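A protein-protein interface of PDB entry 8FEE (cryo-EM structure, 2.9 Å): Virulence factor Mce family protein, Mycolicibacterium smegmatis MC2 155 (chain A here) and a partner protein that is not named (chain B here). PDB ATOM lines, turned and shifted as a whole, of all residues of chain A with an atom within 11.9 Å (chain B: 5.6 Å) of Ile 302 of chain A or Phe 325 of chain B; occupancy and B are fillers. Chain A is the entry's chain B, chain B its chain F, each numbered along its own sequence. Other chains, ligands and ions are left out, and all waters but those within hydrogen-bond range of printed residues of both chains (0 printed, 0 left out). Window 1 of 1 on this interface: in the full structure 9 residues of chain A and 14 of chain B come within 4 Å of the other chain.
N of Gly 301 of chain A is in hydrogen-bond range of O of Phe 306 of chain A. SG of Cys 321 of chain B forms a disulfide with SG of Cys 348 of chain B, at 2.0 Å.
Of the printed residues of chain B, Ile 302 of chain A touches Phe 325 (3.7 Å) and Leu 326 (3.1 Å). Of chain A, only Phe 306 (3.98 Å) comes within 4 Å of Leu 322 of chain B. No residue of chain A comes within 4 Å of Leu 346 of chain B. No residue of chain A comes within 4 Å of Cys 348 of chain B. Printed residues of chain B within 4 Å of Phe 306 of chain A: Leu 322. Of the printed residues of chain A, Leu 342 of chain B touches Arg 298 (3.98 Å). Of the printed residues of chain A, Cys 321 of chain B touches Gly 304 (3.99 Å) and Asp 305 (3.4 Å). Of the printed residues of chain B, Tyr 303 of chain A touches Phe 325 and Leu 326. Printed residues of chain B within 4 Å of Gly 304 of chain A: Cys 321 (3.99 Å) and Phe 325 (3.6 Å). Phe 307 of chain A touches none of the printed residues of chain B.
Hydrophobic or aromatic side chains of chain A that line the printed part of chain B: Tyr 303 and Phe 306. Among the printed residues, 12 pairs touch across the chains. Among the printed residues, no Asp or Glu carboxylate lies within 4 Å of a Lys or Arg side-chain nitrogen of the other chain.
CA of Leu 342 of chain B touches NH1 of Arg 298 of chain A (3.98 Å). Pro 343 of chain B touches Arg 298 of chain A (CD to NH1, 3.4 Å). O of Gly 301 of chain A touches CE1 of Phe 325 of chain B, 3.2 Å away. O of Ile 302 of chain A touches CB of Phe 325 of chain B, 3.7 Å away. O of Tyr 303 of chain A touches CB of Phe 325 of chain B (3.8 Å). Cys 321 of chain B touches Gly 304 of chain A. Phe 325 of chain B touches Gly 304 of chain A (CE1 to O, 3.6 Å). Asp 305 of chain A touches Phe 325 of chain B. CE2 of Phe 306 of chain A touches CD2 of Leu 322 of chain B (3.98 Å).
The backbone NH (N) of Leu 326 of chain B is in hydrogen-bond range of the backbone carbonyl oxygen (O) of Ile 302 of chain A, 3.1 Å away. The backbone NH of Asp 305 of chain A sits at hydrogen-bond distance from the backbone carbonyl oxygen of Cys 321 of chain B (3.4 Å). The backbone carbonyl oxygen of Leu 326 of chain B sits close to the backbone carbonyl oxygen of Tyr 303 of chain A.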
ATOM      1  N   LEU A 293      14.615  11.500 -29.659  1.00  0.00           N
ATOM      2  CA  LEU A 293      13.323  11.294 -29.017  1.00  0.00           C
ATOM      3  C   LEU A 293      13.487  10.923 -27.550  1.00  0.00           C
ATOM      4  O   LEU A 293      12.734  11.408 -26.703  1.00  0.00           O
ATOM      5  CB  LEU A 293      12.523  10.225 -29.760  1.00  0.00           C
ATOM      6  CG  LEU A 293      12.042  10.581 -31.167  1.00  0.00           C
ATOM      7  CD1 LEU A 293      11.056   9.545 -31.670  1.00  0.00           C
ATOM      8  CD2 LEU A 293      11.423  11.966 -31.193  1.00  0.00           C
ATOM      9  N   LYS A 294      14.462  10.070 -27.227  1.00  0.00           N
ATOM     10  CA  LYS A 294      14.716   9.742 -25.824  1.00  0.00           C
ATOM     11  C   LYS A 294      15.157  10.975 -25.042  1.00  0.00           C
ATOM     12  O   LYS A 294      14.695  11.210 -23.913  1.00  0.00           O
ATOM     13  CB  LYS A 294      15.766   8.637 -25.717  1.00  0.00           C
ATOM     14  CG  LYS A 294      15.208   7.234 -25.884  1.00  0.00           C
ATOM     15  CD  LYS A 294      16.315   6.196 -25.936  1.00  0.00           C
ATOM     16  CE  LYS A 294      16.993   6.185 -27.292  1.00  0.00           C
ATOM     17  NZ  LYS A 294      16.037   5.826 -28.374  1.00  0.00           N
ATOM     18  N   ILE A 295      16.040  11.782 -25.639  1.00  0.00           N
ATOM     19  CA  ILE A 295      16.515  13.002 -24.991  1.00  0.00           C
ATOM     20  C   ILE A 295      15.346  13.935 -24.694  1.00  0.00           C
ATOM     21  O   ILE A 295      15.167  14.397 -23.560  1.00  0.00           O
ATOM     22  CB  ILE A 295      17.583  13.686 -25.865  1.00  0.00           C
ATOM     23  CG1 ILE A 295      18.914  12.939 -25.759  1.00  0.00           C
ATOM     24  CG2 ILE A 295      17.756  15.136 -25.470  1.00  0.00           C
ATOM     25  CD1 ILE A 295      20.021  13.543 -26.585  1.00  0.00           C
ATOM     26  N   ILE A 296      14.519  14.208 -25.707  1.00  0.00           N
ATOM     27  CA  ILE A 296      13.429  15.161 -25.522  1.00  0.00           C
ATOM     28  C   ILE A 296      12.368  14.577 -24.596  1.00  0.00           C
ATOM     29  O   ILE A 296      11.693  15.317 -23.872  1.00  0.00           O
ATOM     30  CB  ILE A 296      12.849  15.597 -26.882  1.00  0.00           C
ATOM     31  CG1 ILE A 296      11.901  16.784 -26.705  1.00  0.00           C
ATOM     32  CG2 ILE A 296      12.124  14.461 -27.573  1.00  0.00           C
ATOM     33  CD1 ILE A 296      11.278  17.259 -27.994  1.00  0.00           C
ATOM     34  N   GLY A 297      12.194  13.255 -24.602  1.00  0.00           N
ATOM     35  CA  GLY A 297      11.226  12.644 -23.711  1.00  0.00           C
ATOM     36  C   GLY A 297      11.620  12.783 -22.258  1.00  0.00           C
ATOM     37  O   GLY A 297      10.768  12.997 -21.392  1.00  0.00           O
ATOM     38  N   ARG A 298      12.913  12.662 -21.964  1.00  0.00           N
ATOM     39  CA  ARG A 298      13.326  12.960 -20.600  1.00  0.00           C
ATOM     40  C   ARG A 298      13.483  14.459 -20.353  1.00  0.00           C
ATOM     41  O   ARG A 298      13.658  14.866 -19.200  1.00  0.00           O
ATOM     42  CB  ARG A 298      14.625  12.220 -20.266  1.00  0.00           C
ATOM     43  CG  ARG A 298      14.857  12.055 -18.775  1.00  0.00           C
ATOM     44  CD  ARG A 298      15.782  10.909 -18.446  1.00  0.00           C
ATOM     45  NE  ARG A 298      15.986  10.805 -17.007  1.00  0.00           N
ATOM     46  CZ  ARG A 298      15.141  10.218 -16.172  1.00  0.00           C
ATOM     47  NH1 ARG A 298      14.009   9.684 -16.596  1.00  0.00           N
ATOM     48  NH2 ARG A 298      15.436  10.174 -14.876  1.00  0.00           N
ATOM     49  N   ALA A 299      13.405  15.287 -21.398  1.00  0.00           N
ATOM     50  CA  ALA A 299      13.544  16.730 -21.212  1.00  0.00           C
ATOM     51  C   ALA A 299      12.383  17.307 -20.408  1.00  0.00           C
ATOM     52  O   ALA A 299      12.593  18.056 -19.447  1.00  0.00           O
ATOM     53  CB  ALA A 299      13.658  17.432 -22.563  1.00  0.00           C
ATOM     54  N   GLY A 300      11.151  16.979 -20.784  1.00  0.00           N
ATOM     55  CA  GLY A 300      10.011  17.599 -20.139  1.00  0.00           C
ATOM     56  C   GLY A 300       8.943  16.654 -19.630  1.00  0.00           C
ATOM     57  O   GLY A 300       8.530  15.727 -20.332  1.00  0.00           O
ATOM     58  N   GLY A 301       8.492  16.881 -18.401  1.00  0.00           N
ATOM     59  CA  GLY A 301       7.351  16.180 -17.858  1.00  0.00           C
ATOM     60  C   GLY A 301       7.654  15.005 -16.958  1.00  0.00           C
ATOM     61  O   GLY A 301       6.719  14.303 -16.558  1.00  0.00           O
ATOM     62  N   ILE A 302       8.920  14.762 -16.626  1.00  0.00           N
ATOM     63  CA  ILE A 302       9.236  13.643 -15.746  1.00  0.00           C
ATOM     64  C   ILE A 302       9.095  14.043 -14.284  1.00  0.00           C
ATOM     65  O   ILE A 302       8.553  13.287 -13.472  1.00  0.00           O
ATOM     66  CB  ILE A 302      10.645  13.103 -16.051  1.00  0.00           C
ATOM     67  CG1 ILE A 302      11.646  14.257 -16.166  1.00  0.00           C
ATOM     68  CG2 ILE A 302      10.631  12.269 -17.324  1.00  0.00           C
ATOM     69  CD1 ILE A 302      13.085  13.818 -16.166  1.00  0.00           C
ATOM     70  N   TYR A 303       9.575  15.235 -13.926  1.00  0.00           N
ATOM     71  CA  TYR A 303       9.561  15.664 -12.533  1.00  0.00           C
ATOM     72  C   TYR A 303       8.173  16.081 -12.072  1.00  0.00           C
ATOM     73  O   TYR A 303       7.833  15.899 -10.898  1.00  0.00           O
ATOM     74  CB  TYR A 303      10.544  16.818 -12.342  1.00  0.00           C
ATOM     75  CG  TYR A 303      11.992  16.418 -12.504  1.00  0.00           C
ATOM     76  CD1 TYR A 303      12.409  15.123 -12.239  1.00  0.00           C
ATOM     77  CD2 TYR A 303      12.942  17.337 -12.926  1.00  0.00           C
ATOM     78  CE1 TYR A 303      13.729  14.754 -12.384  1.00  0.00           C
ATOM     79  CE2 TYR A 303      14.265  16.976 -13.075  1.00  0.00           C
ATOM     80  CZ  TYR A 303      14.654  15.683 -12.803  1.00  0.00           C
ATOM     81  OH  TYR A 303      15.972  15.316 -12.951  1.00  0.00           O
ATOM     82  N   GLY A 304       7.367  16.636 -12.971  1.00  0.00           N
ATOM     83  CA  GLY A 304       6.024  17.061 -12.638  1.00  0.00           C
ATOM     84  C   GLY A 304       5.241  17.466 -13.868  1.00  0.00           C
ATOM     85  O   GLY A 304       5.530  17.005 -14.976  1.00  0.00           O
ATOM     86  N   ASP A 305       4.247  18.334 -13.686  1.00  0.00           N
ATOM     87  CA  ASP A 305       3.425  18.790 -14.797  1.00  0.00           C
ATOM     88  C   ASP A 305       4.182  19.739 -15.722  1.00  0.00           C
ATOM     89  O   ASP A 305       3.677  20.071 -16.797  1.00  0.00           O
ATOM     90  CB  ASP A 305       2.167  19.471 -14.244  1.00  0.00           C
ATOM     91  CG  ASP A 305       1.084  19.656 -15.291  1.00  0.00           C
ATOM     92  OD1 ASP A 305       1.196  19.063 -16.381  1.00  0.00           O
ATOM     93  OD2 ASP A 305       0.118  20.399 -15.021  1.00  0.00           O
ATOM     94  N   PHE A 306       5.379  20.163 -15.340  1.00  0.00           N
ATOM     95  CA  PHE A 306       6.090  21.261 -15.976  1.00  0.00           C
ATOM     96  C   PHE A 306       7.175  20.745 -16.918  1.00  0.00           C
ATOM     97  O   PHE A 306       7.560  19.574 -16.888  1.00  0.00           O
ATOM     98  CB  PHE A 306       6.703  22.166 -14.907  1.00  0.00           C
ATOM     99  CG  PHE A 306       7.230  21.418 -13.715  1.00  0.00           C
ATOM    100  CD1 PHE A 306       8.493  20.855 -13.736  1.00  0.00           C
ATOM    101  CD2 PHE A 306       6.459  21.278 -12.572  1.00  0.00           C
ATOM    102  CE1 PHE A 306       8.977  20.164 -12.642  1.00  0.00           C
ATOM    103  CE2 PHE A 306       6.939  20.588 -11.476  1.00  0.00           C
ATOM    104  CZ  PHE A 306       8.199  20.032 -11.510  1.00  0.00           C
ATOM    105  N   PHE A 307       7.668  21.645 -17.763  1.00  0.00           N
ATOM    106  CA  PHE A 307       8.881  21.398 -18.532  1.00  0.00           C
ATOM    107  C   PHE A 307      10.096  21.492 -17.609  1.00  0.00           C
ATOM    108  O   PHE A 307       9.982  21.592 -16.385  1.00  0.00           O
ATOM    109  CB  PHE A 307       8.996  22.384 -19.691  1.00  0.00           C
ATOM    110  CG  PHE A 307       8.322  21.931 -20.950  1.00  0.00           C
ATOM    111  CD1 PHE A 307       7.013  22.284 -21.220  1.00  0.00           C
ATOM    112  CD2 PHE A 307       9.007  21.167 -21.875  1.00  0.00           C
ATOM    113  CE1 PHE A 307       6.398  21.873 -22.386  1.00  0.00           C
ATOM    114  CE2 PHE A 307       8.398  20.753 -23.042  1.00  0.00           C
ATOM    115  CZ  PHE A 307       7.092  21.106 -23.296  1.00  0.00           C
ATOM    116  N   ASN A 308      11.287  21.468 -18.200  1.00  0.00           N
ATOM    117  CA  ASN A 308      12.524  21.712 -17.462  1.00  0.00           C
ATOM    118  C   ASN A 308      13.382  22.658 -18.286  1.00  0.00           C
ATOM    119  O   ASN A 308      13.966  22.249 -19.293  1.00  0.00           O
ATOM    120  CB  ASN A 308      13.265  20.410 -17.173  1.00  0.00           C
ATOM    121  CG  ASN A 308      12.519  19.518 -16.209  1.00  0.00           C
ATOM    122  OD1 ASN A 308      12.575  19.715 -14.995  1.00  0.00           O
ATOM    123  ND2 ASN A 308      11.815  18.527 -16.742  1.00  0.00           N
ATOM    124  N   PHE A 309      13.455  23.916 -17.865  1.00  0.00           N
ATOM    125  CA  PHE A 309      14.260  24.922 -18.537  1.00  0.00           C
ATOM    126  C   PHE A 309      15.460  25.284 -17.672  1.00  0.00           C
ATOM    127  O   PHE A 309      15.348  25.381 -16.446  1.00  0.00           O
ATOM    128  CB  PHE A 309      13.438  26.177 -18.841  1.00  0.00           C
ATOM    129  CG  PHE A 309      12.745  26.143 -20.172  1.00  0.00           C
ATOM    130  CD1 PHE A 309      12.676  24.973 -20.905  1.00  0.00           C
ATOM    131  CD2 PHE A 309      12.170  27.288 -20.694  1.00  0.00           C
ATOM    132  CE1 PHE A 309      12.042  24.945 -22.132  1.00  0.00           C
ATOM    133  CE2 PHE A 309      11.535  27.264 -21.920  1.00  0.00           C
ATOM    134  CZ  PHE A 309      11.471  26.092 -22.639  1.00  0.00           C
ATOM    135  N   ARG A 339      28.043  22.638 -18.094  1.00  0.00           N
ATOM    136  CA  ARG A 339      27.040  21.828 -18.778  1.00  0.00           C
ATOM    137  C   ARG A 339      26.578  22.436 -20.099  1.00  0.00           C
ATOM    138  O   ARG A 339      26.029  21.713 -20.937  1.00  0.00           O
ATOM    139  CB  ARG A 339      25.832  21.605 -17.866  1.00  0.00           C
ATOM    140  CG  ARG A 339      25.275  22.875 -17.261  1.00  0.00           C
ATOM    141  CD  ARG A 339      23.810  22.720 -16.886  1.00  0.00           C
ATOM    142  NE  ARG A 339      22.952  22.548 -18.052  1.00  0.00           N
ATOM    143  CZ  ARG A 339      22.071  21.568 -18.197  1.00  0.00           C
ATOM    144  NH1 ARG A 339      21.888  20.657 -17.256  1.00  0.00           N
ATOM    145  NH2 ARG A 339      21.347  21.507 -19.310  1.00  0.00           N
ATOM    146  N   CYS B 321       0.772  19.762 -10.608  1.00  0.00           N
ATOM    147  CA  CYS B 321       0.548  18.545  -9.843  1.00  0.00           C
ATOM    148  C   CYS B 321       1.799  17.677  -9.839  1.00  0.00           C
ATOM    149  O   CYS B 321       2.479  17.533 -10.859  1.00  0.00           O
ATOM    150  CB  CYS B 321      -0.665  17.791 -10.394  1.00  0.00           C
ATOM    151  SG  CYS B 321      -0.582  17.444 -12.156  1.00  0.00           S
ATOM    152  N   LEU B 322       2.096  17.100  -8.676  1.00  0.00           N
ATOM    153  CA  LEU B 322       3.177  16.138  -8.510  1.00  0.00           C
ATOM    154  C   LEU B 322       2.678  14.713  -8.309  1.00  0.00           C
ATOM    155  O   LEU B 322       3.471  13.834  -7.959  1.00  0.00           O
ATOM    156  CB  LEU B 322       4.072  16.550  -7.339  1.00  0.00           C
ATOM    157  CG  LEU B 322       4.634  17.972  -7.384  1.00  0.00           C
ATOM    158  CD1 LEU B 322       5.556  18.222  -6.201  1.00  0.00           C
ATOM    159  CD2 LEU B 322       5.362  18.225  -8.693  1.00  0.00           C
ATOM    160  N   THR B 323       1.388  14.461  -8.518  1.00  0.00           N
ATOM    161  CA  THR B 323       0.823  13.130  -8.344  1.00  0.00           C
ATOM    162  C   THR B 323       0.904  12.364  -9.655  1.00  0.00           C
ATOM    163  O   THR B 323       0.481  12.862 -10.703  1.00  0.00           O
ATOM    164  CB  THR B 323      -0.629  13.211  -7.874  1.00  0.00           C
ATOM    165  OG1 THR B 323      -1.412  13.893  -8.861  1.00  0.00           O
ATOM    166  CG2 THR B 323      -0.722  13.955  -6.559  1.00  0.00           C
ATOM    167  N   GLY B 324       1.439  11.147  -9.589  1.00  0.00           N
ATOM    168  CA  GLY B 324       1.655  10.346 -10.772  1.00  0.00           C
ATOM    169  C   GLY B 324       2.937  10.637 -11.516  1.00  0.00           C
ATOM    170  O   GLY B 324       3.153  10.061 -12.591  1.00  0.00           O
ATOM    171  N   PHE B 325       3.790  11.506 -10.989  1.00  0.00           N
ATOM    172  CA  PHE B 325       5.073  11.831 -11.589  1.00  0.00           C
ATOM    173  C   PHE B 325       6.197  11.362 -10.672  1.00  0.00           C
ATOM    174  O   PHE B 325       5.964  10.775  -9.612  1.00  0.00           O
ATOM    175  CB  PHE B 325       5.174  13.330 -11.867  1.00  0.00           C
ATOM    176  CG  PHE B 325       4.300  13.797 -12.992  1.00  0.00           C
ATOM    177  CD1 PHE B 325       4.588  13.449 -14.299  1.00  0.00           C
ATOM    178  CD2 PHE B 325       3.197  14.591 -12.743  1.00  0.00           C
ATOM    179  CE1 PHE B 325       3.787  13.882 -15.337  1.00  0.00           C
ATOM    180  CE2 PHE B 325       2.393  15.026 -13.777  1.00  0.00           C
ATOM    181  CZ  PHE B 325       2.688  14.672 -15.075  1.00  0.00           C
ATOM    182  N   LEU B 326       7.427  11.623 -11.100  1.00  0.00           N
ATOM    183  CA  LEU B 326       8.591  11.171 -10.352  1.00  0.00           C
ATOM    184  C   LEU B 326       8.658  11.881  -9.001  1.00  0.00           C
ATOM    185  O   LEU B 326       8.384  13.083  -8.918  1.00  0.00           O
ATOM    186  CB  LEU B 326       9.865  11.436 -11.151  1.00  0.00           C
ATOM    187  CG  LEU B 326      11.153  10.730 -10.731  1.00  0.00           C
ATOM    188  CD1 LEU B 326      11.032   9.232 -10.939  1.00  0.00           C
ATOM    189  CD2 LEU B 326      12.337  11.285 -11.500  1.00  0.00           C
ATOM    190  N   PRO B 327       8.997  11.167  -7.927  1.00  0.00           N
ATOM    191  CA  PRO B 327       9.117  11.816  -6.617  1.00  0.00           C
ATOM    192  C   PRO B 327      10.245  12.836  -6.604  1.00  0.00           C
ATOM    193  O   PRO B 327      11.210  12.734  -7.364  1.00  0.00           O
ATOM    194  CB  PRO B 327       9.405  10.651  -5.664  1.00  0.00           C
ATOM    195  CG  PRO B 327       8.909   9.441  -6.380  1.00  0.00           C
ATOM    196  CD  PRO B 327       9.144   9.706  -7.832  1.00  0.00           C
ATOM    197  N   LEU B 342      13.867   6.695 -19.899  1.00  0.00           N
ATOM    198  CA  LEU B 342      12.641   7.407 -19.562  1.00  0.00           C
ATOM    199  C   LEU B 342      11.584   6.423 -19.068  1.00  0.00           C
ATOM    200  O   LEU B 342      11.349   5.397 -19.714  1.00  0.00           O
ATOM    201  CB  LEU B 342      12.129   8.200 -20.770  1.00  0.00           C
ATOM    202  CG  LEU B 342      11.496   7.572 -22.021  1.00  0.00           C
ATOM    203  CD1 LEU B 342      11.183   8.662 -23.023  1.00  0.00           C
ATOM    204  CD2 LEU B 342      12.356   6.503 -22.680  1.00  0.00           C
ATOM    205  N   PRO B 343      10.954   6.677 -17.924  1.00  0.00           N
ATOM    206  CA  PRO B 343       9.915   5.766 -17.433  1.00  0.00           C
ATOM    207  C   PRO B 343       8.640   5.882 -18.257  1.00  0.00           C
ATOM    208  O   PRO B 343       8.459   6.792 -19.069  1.00  0.00           O
ATOM    209  CB  PRO B 343       9.685   6.224 -15.987  1.00  0.00           C
ATOM    210  CG  PRO B 343      10.861   7.095 -15.653  1.00  0.00           C
ATOM    211  CD  PRO B 343      11.261   7.731 -16.945  1.00  0.00           C
ATOM    212  N   LEU B 346       3.602   7.871 -16.823  1.00  0.00           N
ATOM    213  CA  LEU B 346       3.763   9.089 -16.036  1.00  0.00           C
ATOM    214  C   LEU B 346       2.784  10.139 -16.541  1.00  0.00           C
ATOM    215  O   LEU B 346       2.907  10.615 -17.674  1.00  0.00           O
ATOM    216  CB  LEU B 346       5.197   9.609 -16.113  1.00  0.00           C
ATOM    217  CG  LEU B 346       6.264   8.781 -15.398  1.00  0.00           C
ATOM    218  CD1 LEU B 346       7.616   9.462 -15.499  1.00  0.00           C
ATOM    219  CD2 LEU B 346       5.878   8.558 -13.944  1.00  0.00           C
ATOM    220  N   TYR B 347       1.823  10.503 -15.695  1.00  0.00           N
ATOM    221  CA  TYR B 347       0.934  11.624 -15.968  1.00  0.00           C
ATOM    222  C   TYR B 347       0.284  12.049 -14.659  1.00  0.00           C
ATOM    223  O   TYR B 347       0.360  11.352 -13.644  1.00  0.00           O
ATOM    224  CB  TYR B 347      -0.117  11.280 -17.032  1.00  0.00           C
ATOM    225  CG  TYR B 347      -0.990  10.088 -16.712  1.00  0.00           C
ATOM    226  CD1 TYR B 347      -0.591   8.800 -17.043  1.00  0.00           C
ATOM    227  CD2 TYR B 347      -2.224  10.254 -16.099  1.00  0.00           C
ATOM    228  CE1 TYR B 347      -1.390   7.710 -16.758  1.00  0.00           C
ATOM    229  CE2 TYR B 347      -3.028   9.170 -15.810  1.00  0.00           C
ATOM    230  CZ  TYR B 347      -2.608   7.902 -16.143  1.00  0.00           C
ATOM    231  OH  TYR B 347      -3.411   6.823 -15.855  1.00  0.00           O
ATOM    232  N   CYS B 348      -0.343  13.223 -14.698  1.00  0.00           N
ATOM    233  CA  CYS B 348      -0.996  13.793 -13.526  1.00  0.00           C
ATOM    234  C   CYS B 348      -2.164  12.919 -13.077  1.00  0.00           C
ATOM    235  O   CYS B 348      -3.009  12.527 -13.888  1.00  0.00           O
ATOM    236  CB  CYS B 348      -1.461  15.205 -13.865  1.00  0.00           C
ATOM    237  SG  CYS B 348      -2.153  16.218 -12.561  1.00  0.00           S
ATOM    238  N   LYS B 349      -2.212  12.616 -11.780  1.00  0.00           N
ATOM    239  CA  LYS B 349      -3.181  11.661 -11.251  1.00  0.00           C
ATOM    240  C   LYS B 349      -4.197  12.300 -10.311  1.00  0.00           C
ATOM    241  O   LYS B 349      -4.474  11.757  -9.238  1.00  0.00           O
ATOM    242  CB  LYS B 349      -2.465  10.528 -10.514  1.00  0.00           C
ATOM    243  CG  LYS B 349      -1.741   9.534 -11.402  1.00  0.00           C
ATOM    244  CD  LYS B 349      -2.701   8.678 -12.201  1.00  0.00           C
ATOM    245  CE  LYS B 349      -1.985   7.471 -12.779  1.00  0.00           C
ATOM    246  NZ  LYS B 349      -0.775   7.865 -13.547  1.00  0.00           N
